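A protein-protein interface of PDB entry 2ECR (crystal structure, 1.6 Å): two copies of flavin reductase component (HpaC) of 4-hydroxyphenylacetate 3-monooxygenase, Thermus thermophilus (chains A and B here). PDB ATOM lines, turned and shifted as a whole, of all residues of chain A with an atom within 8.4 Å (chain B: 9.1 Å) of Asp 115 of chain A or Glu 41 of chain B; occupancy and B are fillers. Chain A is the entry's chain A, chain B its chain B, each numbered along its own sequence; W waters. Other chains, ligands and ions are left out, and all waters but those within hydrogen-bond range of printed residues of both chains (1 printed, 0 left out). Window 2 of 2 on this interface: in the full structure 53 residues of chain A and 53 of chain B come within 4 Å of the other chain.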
ATOM      1  N   MET A   1      12.689  35.787  37.991  1.00  0.00           N
ATOM      2  CA  MET A   1      12.816  34.310  37.854  1.00  0.00           C
ATOM      3  C   MET A   1      13.108  33.926  36.405  1.00  0.00           C
ATOM      4  O   MET A   1      12.795  34.673  35.479  1.00  0.00           O
ATOM      5  CB  MET A   1      11.517  33.622  38.290  1.00  0.00           C
ATOM      6  CG  MET A   1      11.084  33.903  39.721  1.00  0.00           C
ATOM      7  SD  MET A   1      12.219  33.227  40.948  1.00  0.00           S
ATOM      8  CE  MET A   1      11.725  31.496  40.956  1.00  0.00           C
ATOM      9  N   LYS A   2      13.714  32.758  36.225  1.00  0.00           N
ATOM     10  CA  LYS A   2      14.026  32.234  34.897  1.00  0.00           C
ATOM     11  C   LYS A   2      14.836  33.174  34.003  1.00  0.00           C
ATOM     12  O   LYS A   2      14.668  33.159  32.784  1.00  0.00           O
ATOM     13  CB  LYS A   2      12.727  31.874  34.169  1.00  0.00           C
ATOM     14  CG  LYS A   2      11.804  30.909  34.910  1.00  0.00           C
ATOM     15  CD  LYS A   2      12.476  29.574  35.187  1.00  0.00           C
ATOM     16  CE  LYS A   2      11.445  28.520  35.573  1.00  0.00           C
ATOM     17  NZ  LYS A   2      10.570  28.976  36.687  1.00  0.00           N
ATOM     18  N   PHE A   5      16.957  31.240  31.335  1.00  0.00           N
ATOM     19  CA  PHE A   5      16.067  30.611  30.368  1.00  0.00           C
ATOM     20  C   PHE A   5      15.516  31.653  29.395  1.00  0.00           C
ATOM     21  O   PHE A   5      15.471  31.422  28.182  1.00  0.00           O
ATOM     22  CB  PHE A   5      14.924  29.917  31.111  1.00  0.00           C
ATOM     23  CG  PHE A   5      13.905  29.284  30.211  1.00  0.00           C
ATOM     24  CD1 PHE A   5      14.287  28.383  29.221  1.00  0.00           C
ATOM     25  CD2 PHE A   5      12.554  29.567  30.375  1.00  0.00           C
ATOM     26  CE1 PHE A   5      13.334  27.772  28.410  1.00  0.00           C
ATOM     27  CE2 PHE A   5      11.596  28.959  29.568  1.00  0.00           C
ATOM     28  CZ  PHE A   5      11.991  28.059  28.584  1.00  0.00           C
ATOM     29  N   LYS A   6      15.101  32.800  29.931  1.00  0.00           N
ATOM     30  CA  LYS A   6      14.562  33.873  29.103  1.00  0.00           C
ATOM     31  C   LYS A   6      15.633  34.405  28.158  1.00  0.00           C
ATOM     32  O   LYS A   6      15.339  34.780  27.018  1.00  0.00           O
ATOM     33  CB  LYS A   6      14.026  35.002  29.984  1.00  0.00           C
ATOM     34  CG  LYS A   6      12.806  34.614  30.814  1.00  0.00           C
ATOM     35  CD  LYS A   6      12.373  35.767  31.712  1.00  0.00           C
ATOM     36  CE  LYS A   6      11.204  35.375  32.600  1.00  0.00           C
ATOM     37  NZ  LYS A   6      10.778  36.509  33.464  1.00  0.00           N
ATOM     38  N   ALA A  48       2.292  28.071  19.610  1.00  0.00           N
ATOM     39  CA  ALA A  48       2.104  28.114  21.053  1.00  0.00           C
ATOM     40  C   ALA A  48       1.275  29.372  21.274  1.00  0.00           C
ATOM     41  O   ALA A  48       1.699  30.471  20.907  1.00  0.00           O
ATOM     42  CB  ALA A  48       3.434  28.228  21.778  1.00  0.00           C
ATOM     43  N   VAL A  49       0.088  29.203  21.848  1.00  0.00           N
ATOM     44  CA  VAL A  49      -0.812  30.315  22.116  1.00  0.00           C
ATOM     45  C   VAL A  49      -1.025  30.411  23.620  1.00  0.00           C
ATOM     46  O   VAL A  49      -1.344  29.425  24.272  1.00  0.00           O
ATOM     47  CB  VAL A  49      -2.182  30.107  21.417  1.00  0.00           C
ATOM     48  CG1 VAL A  49      -3.159  31.208  21.826  1.00  0.00           C
ATOM     49  CG2 VAL A  49      -1.999  30.106  19.910  1.00  0.00           C
ATOM     50  N   SER A  50      -0.844  31.603  24.170  1.00  0.00           N
ATOM     51  CA  SER A  50      -1.017  31.794  25.600  1.00  0.00           C
ATOM     52  C   SER A  50      -2.403  31.388  26.080  1.00  0.00           C
ATOM     53  O   SER A  50      -3.409  31.651  25.419  1.00  0.00           O
ATOM     54  CB  SER A  50      -0.769  33.255  25.970  1.00  0.00           C
ATOM     55  OG  SER A  50      -1.002  33.470  27.354  1.00  0.00           O
ATOM     56  N   GLU A  51      -2.446  30.738  27.235  1.00  0.00           N
ATOM     57  CA  GLU A  51      -3.709  30.323  27.820  1.00  0.00           C
ATOM     58  C   GLU A  51      -4.485  31.566  28.259  1.00  0.00           C
ATOM     59  O   GLU A  51      -5.679  31.490  28.553  1.00  0.00           O
ATOM     60  CB  GLU A  51      -3.452  29.395  29.010  1.00  0.00           C
ATOM     61  CG  GLU A  51      -2.883  28.024  28.620  1.00  0.00           C
ATOM     62  CD  GLU A  51      -3.935  27.066  28.075  1.00  0.00           C
ATOM     63  OE1 GLU A  51      -5.129  27.437  28.032  1.00  0.00           O
ATOM     64  OE2 GLU A  51      -3.571  25.929  27.696  1.00  0.00           O
ATOM     65  N   ARG A  52      -3.797  32.707  28.299  1.00  0.00           N
ATOM     66  CA  ARG A  52      -4.404  33.987  28.679  1.00  0.00           C
ATOM     67  C   ARG A  52      -4.931  34.749  27.464  1.00  0.00           C
ATOM     68  O   ARG A  52      -5.666  35.727  27.608  1.00  0.00           O
ATOM     69  CB  ARG A  52      -3.384  34.900  29.368  1.00  0.00           C
ATOM     70  CG  ARG A  52      -3.238  34.751  30.872  1.00  0.00           C
ATOM     71  CD  ARG A  52      -2.388  33.559  31.246  1.00  0.00           C
ATOM     72  NE  ARG A  52      -3.199  32.421  31.657  1.00  0.00           N
ATOM     73  CZ  ARG A  52      -2.696  31.299  32.156  1.00  0.00           C
ATOM     74  NH1 ARG A  52      -1.385  31.169  32.301  1.00  0.00           N
ATOM     75  NH2 ARG A  52      -3.504  30.312  32.520  1.00  0.00           N
ATOM     76  N   ALA A  53      -4.550  34.307  26.271  1.00  0.00           N
ATOM     77  CA  ALA A  53      -4.944  34.986  25.038  1.00  0.00           C
ATOM     78  C   ALA A  53      -6.430  34.999  24.715  1.00  0.00           C
ATOM     79  O   ALA A  53      -7.107  33.977  24.791  1.00  0.00           O
ATOM     80  CB  ALA A  53      -4.175  34.402  23.861  1.00  0.00           C
ATOM     81  N   LEU A  56      -7.457  32.558  21.843  1.00  0.00           N
ATOM     82  CA  LEU A  56      -7.629  31.127  22.065  1.00  0.00           C
ATOM     83  C   LEU A  56      -9.060  30.594  22.010  1.00  0.00           C
ATOM     84  O   LEU A  56      -9.359  29.698  21.219  1.00  0.00           O
ATOM     85  CB  LEU A  56      -6.956  30.709  23.381  1.00  0.00           C
ATOM     86  CG  LEU A  56      -6.822  29.194  23.587  1.00  0.00           C
ATOM     87  CD1 LEU A  56      -6.191  28.554  22.354  1.00  0.00           C
ATOM     88  CD2 LEU A  56      -5.977  28.911  24.821  1.00  0.00           C
ATOM     89  N   PRO A 112      -1.894  20.287  25.791  1.00  0.00           N
ATOM     90  CA  PRO A 112      -1.497  21.130  26.921  1.00  0.00           C
ATOM     91  C   PRO A 112      -0.076  21.627  26.671  1.00  0.00           C
ATOM     92  O   PRO A 112       0.711  20.949  26.008  1.00  0.00           O
ATOM     93  CB  PRO A 112      -1.555  20.170  28.104  1.00  0.00           C
ATOM     94  CG  PRO A 112      -2.655  19.232  27.722  1.00  0.00           C
ATOM     95  CD  PRO A 112      -2.358  18.966  26.259  1.00  0.00           C
ATOM     96  N   GLY A 113       0.252  22.801  27.197  1.00  0.00           N
ATOM     97  CA  GLY A 113       1.592  23.328  27.006  1.00  0.00           C
ATOM     98  C   GLY A 113       2.022  24.251  28.127  1.00  0.00           C
ATOM     99  O   GLY A 113       2.659  25.277  27.883  1.00  0.00           O
ATOM    100  N   GLY A 114       1.674  23.894  29.359  1.00  0.00           N
ATOM    101  CA  GLY A 114       2.038  24.731  30.489  1.00  0.00           C
ATOM    102  C   GLY A 114       1.158  25.964  30.512  1.00  0.00           C
ATOM    103  O   GLY A 114      -0.068  25.842  30.595  1.00  0.00           O
ATOM    104  N   ASP A 115       1.762  27.151  30.440  1.00  0.00           N
ATOM    105  CA  ASP A 115       0.969  28.373  30.431  1.00  0.00           C
ATOM    106  C   ASP A 115       0.523  28.717  29.012  1.00  0.00           C
ATOM    107  O   ASP A 115      -0.111  29.747  28.782  1.00  0.00           O
ATOM    108  CB  ASP A 115       1.723  29.559  31.066  1.00  0.00           C
ATOM    109  CG  ASP A 115       3.095  29.790  30.469  1.00  0.00           C
ATOM    110  OD1 ASP A 115       3.260  29.632  29.242  1.00  0.00           O
ATOM    111  OD2 ASP A 115       4.011  30.160  31.239  1.00  0.00           O
ATOM    112  N   HIS A 116       0.851  27.844  28.063  1.00  0.00           N
ATOM    113  CA  HIS A 116       0.447  28.022  26.665  1.00  0.00           C
ATOM    114  C   HIS A 116      -0.271  26.763  26.191  1.00  0.00           C
ATOM    115  O   HIS A 116      -0.220  25.723  26.844  1.00  0.00           O
ATOM    116  CB  HIS A 116       1.657  28.244  25.750  1.00  0.00           C
ATOM    117  CG  HIS A 116       2.139  29.661  25.697  1.00  0.00           C
ATOM    118  ND1 HIS A 116       2.676  30.308  26.787  1.00  0.00           N
ATOM    119  CD2 HIS A 116       2.185  30.547  24.673  1.00  0.00           C
ATOM    120  CE1 HIS A 116       3.035  31.532  26.440  1.00  0.00           C
ATOM    121  NE2 HIS A 116       2.748  31.702  25.161  1.00  0.00           N
ATOM    122  N   ARG A 117      -0.945  26.864  25.051  1.00  0.00           N
ATOM    123  CA  ARG A 117      -1.623  25.714  24.470  1.00  0.00           C
ATOM    124  C   ARG A 117      -0.918  25.416  23.155  1.00  0.00           C
ATOM    125  O   ARG A 117      -0.574  26.337  22.411  1.00  0.00           O
ATOM    126  CB  ARG A 117      -3.094  26.022  24.169  1.00  0.00           C
ATOM    127  CG  ARG A 117      -3.891  24.810  23.677  1.00  0.00           C
ATOM    128  CD  ARG A 117      -4.286  23.910  24.833  1.00  0.00           C
ATOM    129  NE  ARG A 117      -5.104  24.654  25.786  1.00  0.00           N
ATOM    130  CZ  ARG A 117      -6.390  24.939  25.603  1.00  0.00           C
ATOM    131  NH1 ARG A 117      -7.018  24.528  24.510  1.00  0.00           N
ATOM    132  NH2 ARG A 117      -7.036  25.678  26.494  1.00  0.00           N
ATOM    133  N   ILE A 118      -0.683  24.141  22.873  1.00  0.00           N
ATOM    134  CA  ILE A 118      -0.062  23.776  21.606  1.00  0.00           C
ATOM    135  C   ILE A 118      -1.208  23.672  20.614  1.00  0.00           C
ATOM    136  O   ILE A 118      -2.146  22.896  20.810  1.00  0.00           O
ATOM    137  CB  ILE A 118       0.670  22.425  21.682  1.00  0.00           C
ATOM    138  CG1 ILE A 118       1.851  22.529  22.650  1.00  0.00           C
ATOM    139  CG2 ILE A 118       1.154  22.024  20.293  1.00  0.00           C
ATOM    140  CD1 ILE A 118       2.596  21.222  22.856  1.00  0.00           C
ATOM    141  N   SER B  37       9.650  28.241  21.742  1.00  0.00           N
ATOM    142  CA  SER B  37       9.459  28.331  23.177  1.00  0.00           C
ATOM    143  C   SER B  37       8.006  27.944  23.375  1.00  0.00           C
ATOM    144  O   SER B  37       7.186  28.109  22.469  1.00  0.00           O
ATOM    145  CB  SER B  37       9.706  29.759  23.667  1.00  0.00           C
ATOM    146  OG  SER B  37       8.792  30.664  23.083  1.00  0.00           O
ATOM    147  N   LEU B  38       7.677  27.430  24.549  1.00  0.00           N
ATOM    148  CA  LEU B  38       6.309  27.019  24.798  1.00  0.00           C
ATOM    149  C   LEU B  38       5.715  27.589  26.070  1.00  0.00           C
ATOM    150  O   LEU B  38       4.634  28.169  26.040  1.00  0.00           O
ATOM    151  CB  LEU B  38       6.222  25.489  24.829  1.00  0.00           C
ATOM    152  CG  LEU B  38       4.838  24.899  25.128  1.00  0.00           C
ATOM    153  CD1 LEU B  38       3.815  25.412  24.113  1.00  0.00           C
ATOM    154  CD2 LEU B  38       4.922  23.380  25.084  1.00  0.00           C
ATOM    155  N   SER B  39       6.432  27.444  27.180  1.00  0.00           N
ATOM    156  CA  SER B  39       5.929  27.910  28.463  1.00  0.00           C
ATOM    157  C   SER B  39       7.024  28.440  29.381  1.00  0.00           C
ATOM    158  O   SER B  39       8.183  28.063  29.253  1.00  0.00           O
ATOM    159  CB  SER B  39       5.196  26.754  29.153  1.00  0.00           C
ATOM    160  OG  SER B  39       4.679  27.139  30.406  1.00  0.00           O
ATOM    161  N   LEU B  40       6.643  29.324  30.300  1.00  0.00           N
ATOM    162  CA  LEU B  40       7.589  29.886  31.260  1.00  0.00           C
ATOM    163  C   LEU B  40       7.396  29.155  32.588  1.00  0.00           C
ATOM    164  O   LEU B  40       8.365  28.765  33.236  1.00  0.00           O
ATOM    165  CB  LEU B  40       7.341  31.390  31.441  1.00  0.00           C
ATOM    166  CG  LEU B  40       8.234  32.112  32.455  1.00  0.00           C
ATOM    167  CD1 LEU B  40       9.690  31.998  32.024  1.00  0.00           C
ATOM    168  CD2 LEU B  40       7.822  33.577  32.559  1.00  0.00           C
ATOM    169  N   GLU B  41       6.139  28.958  32.976  1.00  0.00           N
ATOM    170  CA  GLU B  41       5.803  28.259  34.215  1.00  0.00           C
ATOM    171  C   GLU B  41       4.845  27.101  33.928  1.00  0.00           C
ATOM    172  O   GLU B  41       3.640  27.314  33.797  1.00  0.00           O
ATOM    173  CB  GLU B  41       5.127  29.210  35.209  1.00  0.00           C
ATOM    174  CG  GLU B  41       5.931  30.443  35.584  1.00  0.00           C
ATOM    175  CD  GLU B  41       5.167  31.365  36.524  1.00  0.00           C
ATOM    176  OE1 GLU B  41       5.730  32.401  36.936  1.00  0.00           O
ATOM    177  OE2 GLU B  41       4.001  31.053  36.851  1.00  0.00           O
ATOM    178  N   PRO B  42       5.361  25.863  33.825  1.00  0.00           N
ATOM    179  CA  PRO B  42       6.769  25.476  33.952  1.00  0.00           C
ATOM    180  C   PRO B  42       7.542  25.858  32.693  1.00  0.00           C
ATOM    181  O   PRO B  42       6.940  26.195  31.676  1.00  0.00           O
ATOM    182  CB  PRO B  42       6.689  23.968  34.143  1.00  0.00           C
ATOM    183  CG  PRO B  42       5.523  23.600  33.283  1.00  0.00           C
ATOM    184  CD  PRO B  42       4.514  24.669  33.643  1.00  0.00           C
ATOM    185  N   PRO B  43       8.883  25.810  32.749  1.00  0.00           N
ATOM    186  CA  PRO B  43       9.722  26.159  31.597  1.00  0.00           C
ATOM    187  C   PRO B  43       9.718  25.050  30.551  1.00  0.00           C
ATOM    188  O   PRO B  43      10.343  24.009  30.729  1.00  0.00           O
ATOM    189  CB  PRO B  43      11.092  26.375  32.231  1.00  0.00           C
ATOM    190  CG  PRO B  43      11.098  25.364  33.333  1.00  0.00           C
ATOM    191  CD  PRO B  43       9.714  25.525  33.934  1.00  0.00           C
ATOM    192  N   LEU B  44       9.008  25.282  29.454  1.00  0.00           N
ATOM    193  CA  LEU B  44       8.902  24.276  28.406  1.00  0.00           C
ATOM    194  C   LEU B  44       9.248  24.800  27.024  1.00  0.00           C
ATOM    195  O   LEU B  44       9.049  25.978  26.722  1.00  0.00           O
ATOM    196  CB  LEU B  44       7.473  23.732  28.343  1.00  0.00           C
ATOM    197  CG  LEU B  44       6.779  23.181  29.586  1.00  0.00           C
ATOM    198  CD1 LEU B  44       5.337  22.855  29.239  1.00  0.00           C
ATOM    199  CD2 LEU B  44       7.498  21.938  30.083  1.00  0.00           C
ATOM    200  N   HIS B 108       9.138  15.888  28.699  1.00  0.00           N
ATOM    201  CA  HIS B 108       7.884  16.218  29.361  1.00  0.00           C
ATOM    202  C   HIS B 108       6.711  15.525  28.673  1.00  0.00           C
ATOM    203  O   HIS B 108       5.817  14.996  29.337  1.00  0.00           O
ATOM    204  CB  HIS B 108       7.665  17.732  29.340  1.00  0.00           C
ATOM    205  CG  HIS B 108       6.453  18.181  30.097  1.00  0.00           C
ATOM    206  ND1 HIS B 108       6.382  18.149  31.474  1.00  0.00           N
ATOM    207  CD2 HIS B 108       5.264  18.668  29.671  1.00  0.00           C
ATOM    208  CE1 HIS B 108       5.202  18.598  31.862  1.00  0.00           C
ATOM    209  NE2 HIS B 108       4.503  18.920  30.788  1.00  0.00           N
ATOM    210  N   LEU B 122      11.138  19.886  29.394  1.00  0.00           N
ATOM    211  CA  LEU B 122      11.079  20.714  30.591  1.00  0.00           C
ATOM    212  C   LEU B 122      12.528  21.119  30.821  1.00  0.00           C
ATOM    213  O   LEU B 122      13.382  20.266  31.058  1.00  0.00           O
ATOM    214  CB  LEU B 122      10.577  19.901  31.785  1.00  0.00           C
ATOM    215  CG  LEU B 122      10.664  20.600  33.143  1.00  0.00           C
ATOM    216  CD1 LEU B 122       9.609  21.683  33.219  1.00  0.00           C
ATOM    217  CD2 LEU B 122      10.466  19.587  34.256  1.00  0.00           C
HETATM  218  O   HOH W   1       5.803  30.711  24.144  1.00  0.00           O
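The side-chain carboxylate (OD2) of Asp 115 of chain A is in hydrogen-bond range of the backbone NH (N) of Leu 40 of chain B (2.9 Å).
The side-chain hydroxyl (OG) of Ser 39 of chain B is in hydrogen-bond range of the backbone NH (N) of Asp 115 of chain A (2.9 Å).
O of Leu 38 of chain B sits close to ND1 of His 116 of chain A, 3.0 Å away.
The side-chain carboxylate (OD2) of Asp 115 of chain A lies within hydrogen-bond range of the backbone NH (N) of Glu 41 of chain B, 3.0 Å away.
The backbone carbonyl oxygen (O) of Ser 39 of chain B lies within hydrogen-bond range of the backbone NH (N) of Leu 44 of chain B.
ND1 of His 116 of chain A sits at hydrogen-bond distance from OD1 of Asp 115 of chain A (2.6 Å).
The backbone NH of Leu 38 of chain B sits at hydrogen-bond distance from the backbone carbonyl oxygen of Leu 44 of chain B (3.0 Å).
The backbone NH (N) of Glu 51 of chain A sits at hydrogen-bond distance from the backbone carbonyl oxygen (O) of Asp 115 of chain A.
The side-chain hydroxyl (OG) of Ser 39 of chain B sits at hydrogen-bond distance from the backbone NH (N) of Glu 41 of chain B (3.5 Å).
The side-chain hydroxyl (OG) of Ser 39 of chain B is in hydrogen-bond range of the backbone carbonyl oxygen (O) of Pro 42 of chain B.
CB of Lys 2 of chain A touches CD1 of Leu 40 of chain B, 3.7 Å away.
Ser 39 of chain B touches Phe 5 of chain A (O to CE2, 3.5 Å).
Leu 40 of chain B touches Lys 6 of chain A (CD1 to CE, 3.7 Å).
Ala 48 of chain A touches Ser 37 of chain B.
Leu 38 of chain B touches Ala 48 of chain A (CD1 to CB, 3.7 Å).
O of Gly 113 of chain A touches CG of Leu 38 of chain B (3.5 Å).
C of Gly 113 of chain A touches CD1 of Leu 44 of chain B, at 3.8 Å.
Gly 114 of chain A touches Ser 39 of chain B (CA to OG, 3.6 Å).
Leu 44 of chain B touches Gly 114 of chain A (CD1 to N, 3.8 Å).
Leu 38 of chain B touches Asp 115 of chain A (O to OD1, 3.8 Å).
Asp 115 of chain A touches just these residues of chain B: Leu 38, Ser 39, Leu 40 and Glu 41.
Glu 41 of chain B touches just one residue of chain A: Asp 115 (3.0 Å).
Of chain B, only Leu 38 comes within 4 Å of His 116 of chain A.
Of the printed residues of chain B, Phe 5 of chain A touches Ser 39 (3.5 Å) and Pro 43 (3.7 Å).
Of the printed residues of chain A, Ser 37 of chain B touches Ala 48.
The nearest residue of chain A that does not touch Glu 41 of chain B is Gly 114 of chain A (4.3 Å).
The nearest printed residue of chain B that does not touch Gly 114 of chain A is Pro 42 of chain B (4.01 Å).
Hydrophobic or aromatic side chains of chain A within 4 Å of the printed part of chain B: Phe 5, Ala 48, His 116 and Ile 118.
Along chain A the printed residues that touch a printed residue of chain B span positions 2 to 118.
Hydrophobic or aromatic side chains of chain B within 4 Å of the printed part of chain A: Leu 38, Leu 40, Pro 43 and Leu 44.
Along chain B the printed residues that touch a printed residue of chain A span positions 37 to 44.
No position is printed for both chains.
Of the 18 pairs that touch across the chains among the printed residues, none has its exchanged pair printed and touching as well.
Water W1 lies within hydrogen-bond range of OG of Ser 37 of chain B (3.2 Å), NE2 of His 116 of chain A (3.4 Å) and O of Leu 38 of chain B (3.4 Å).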
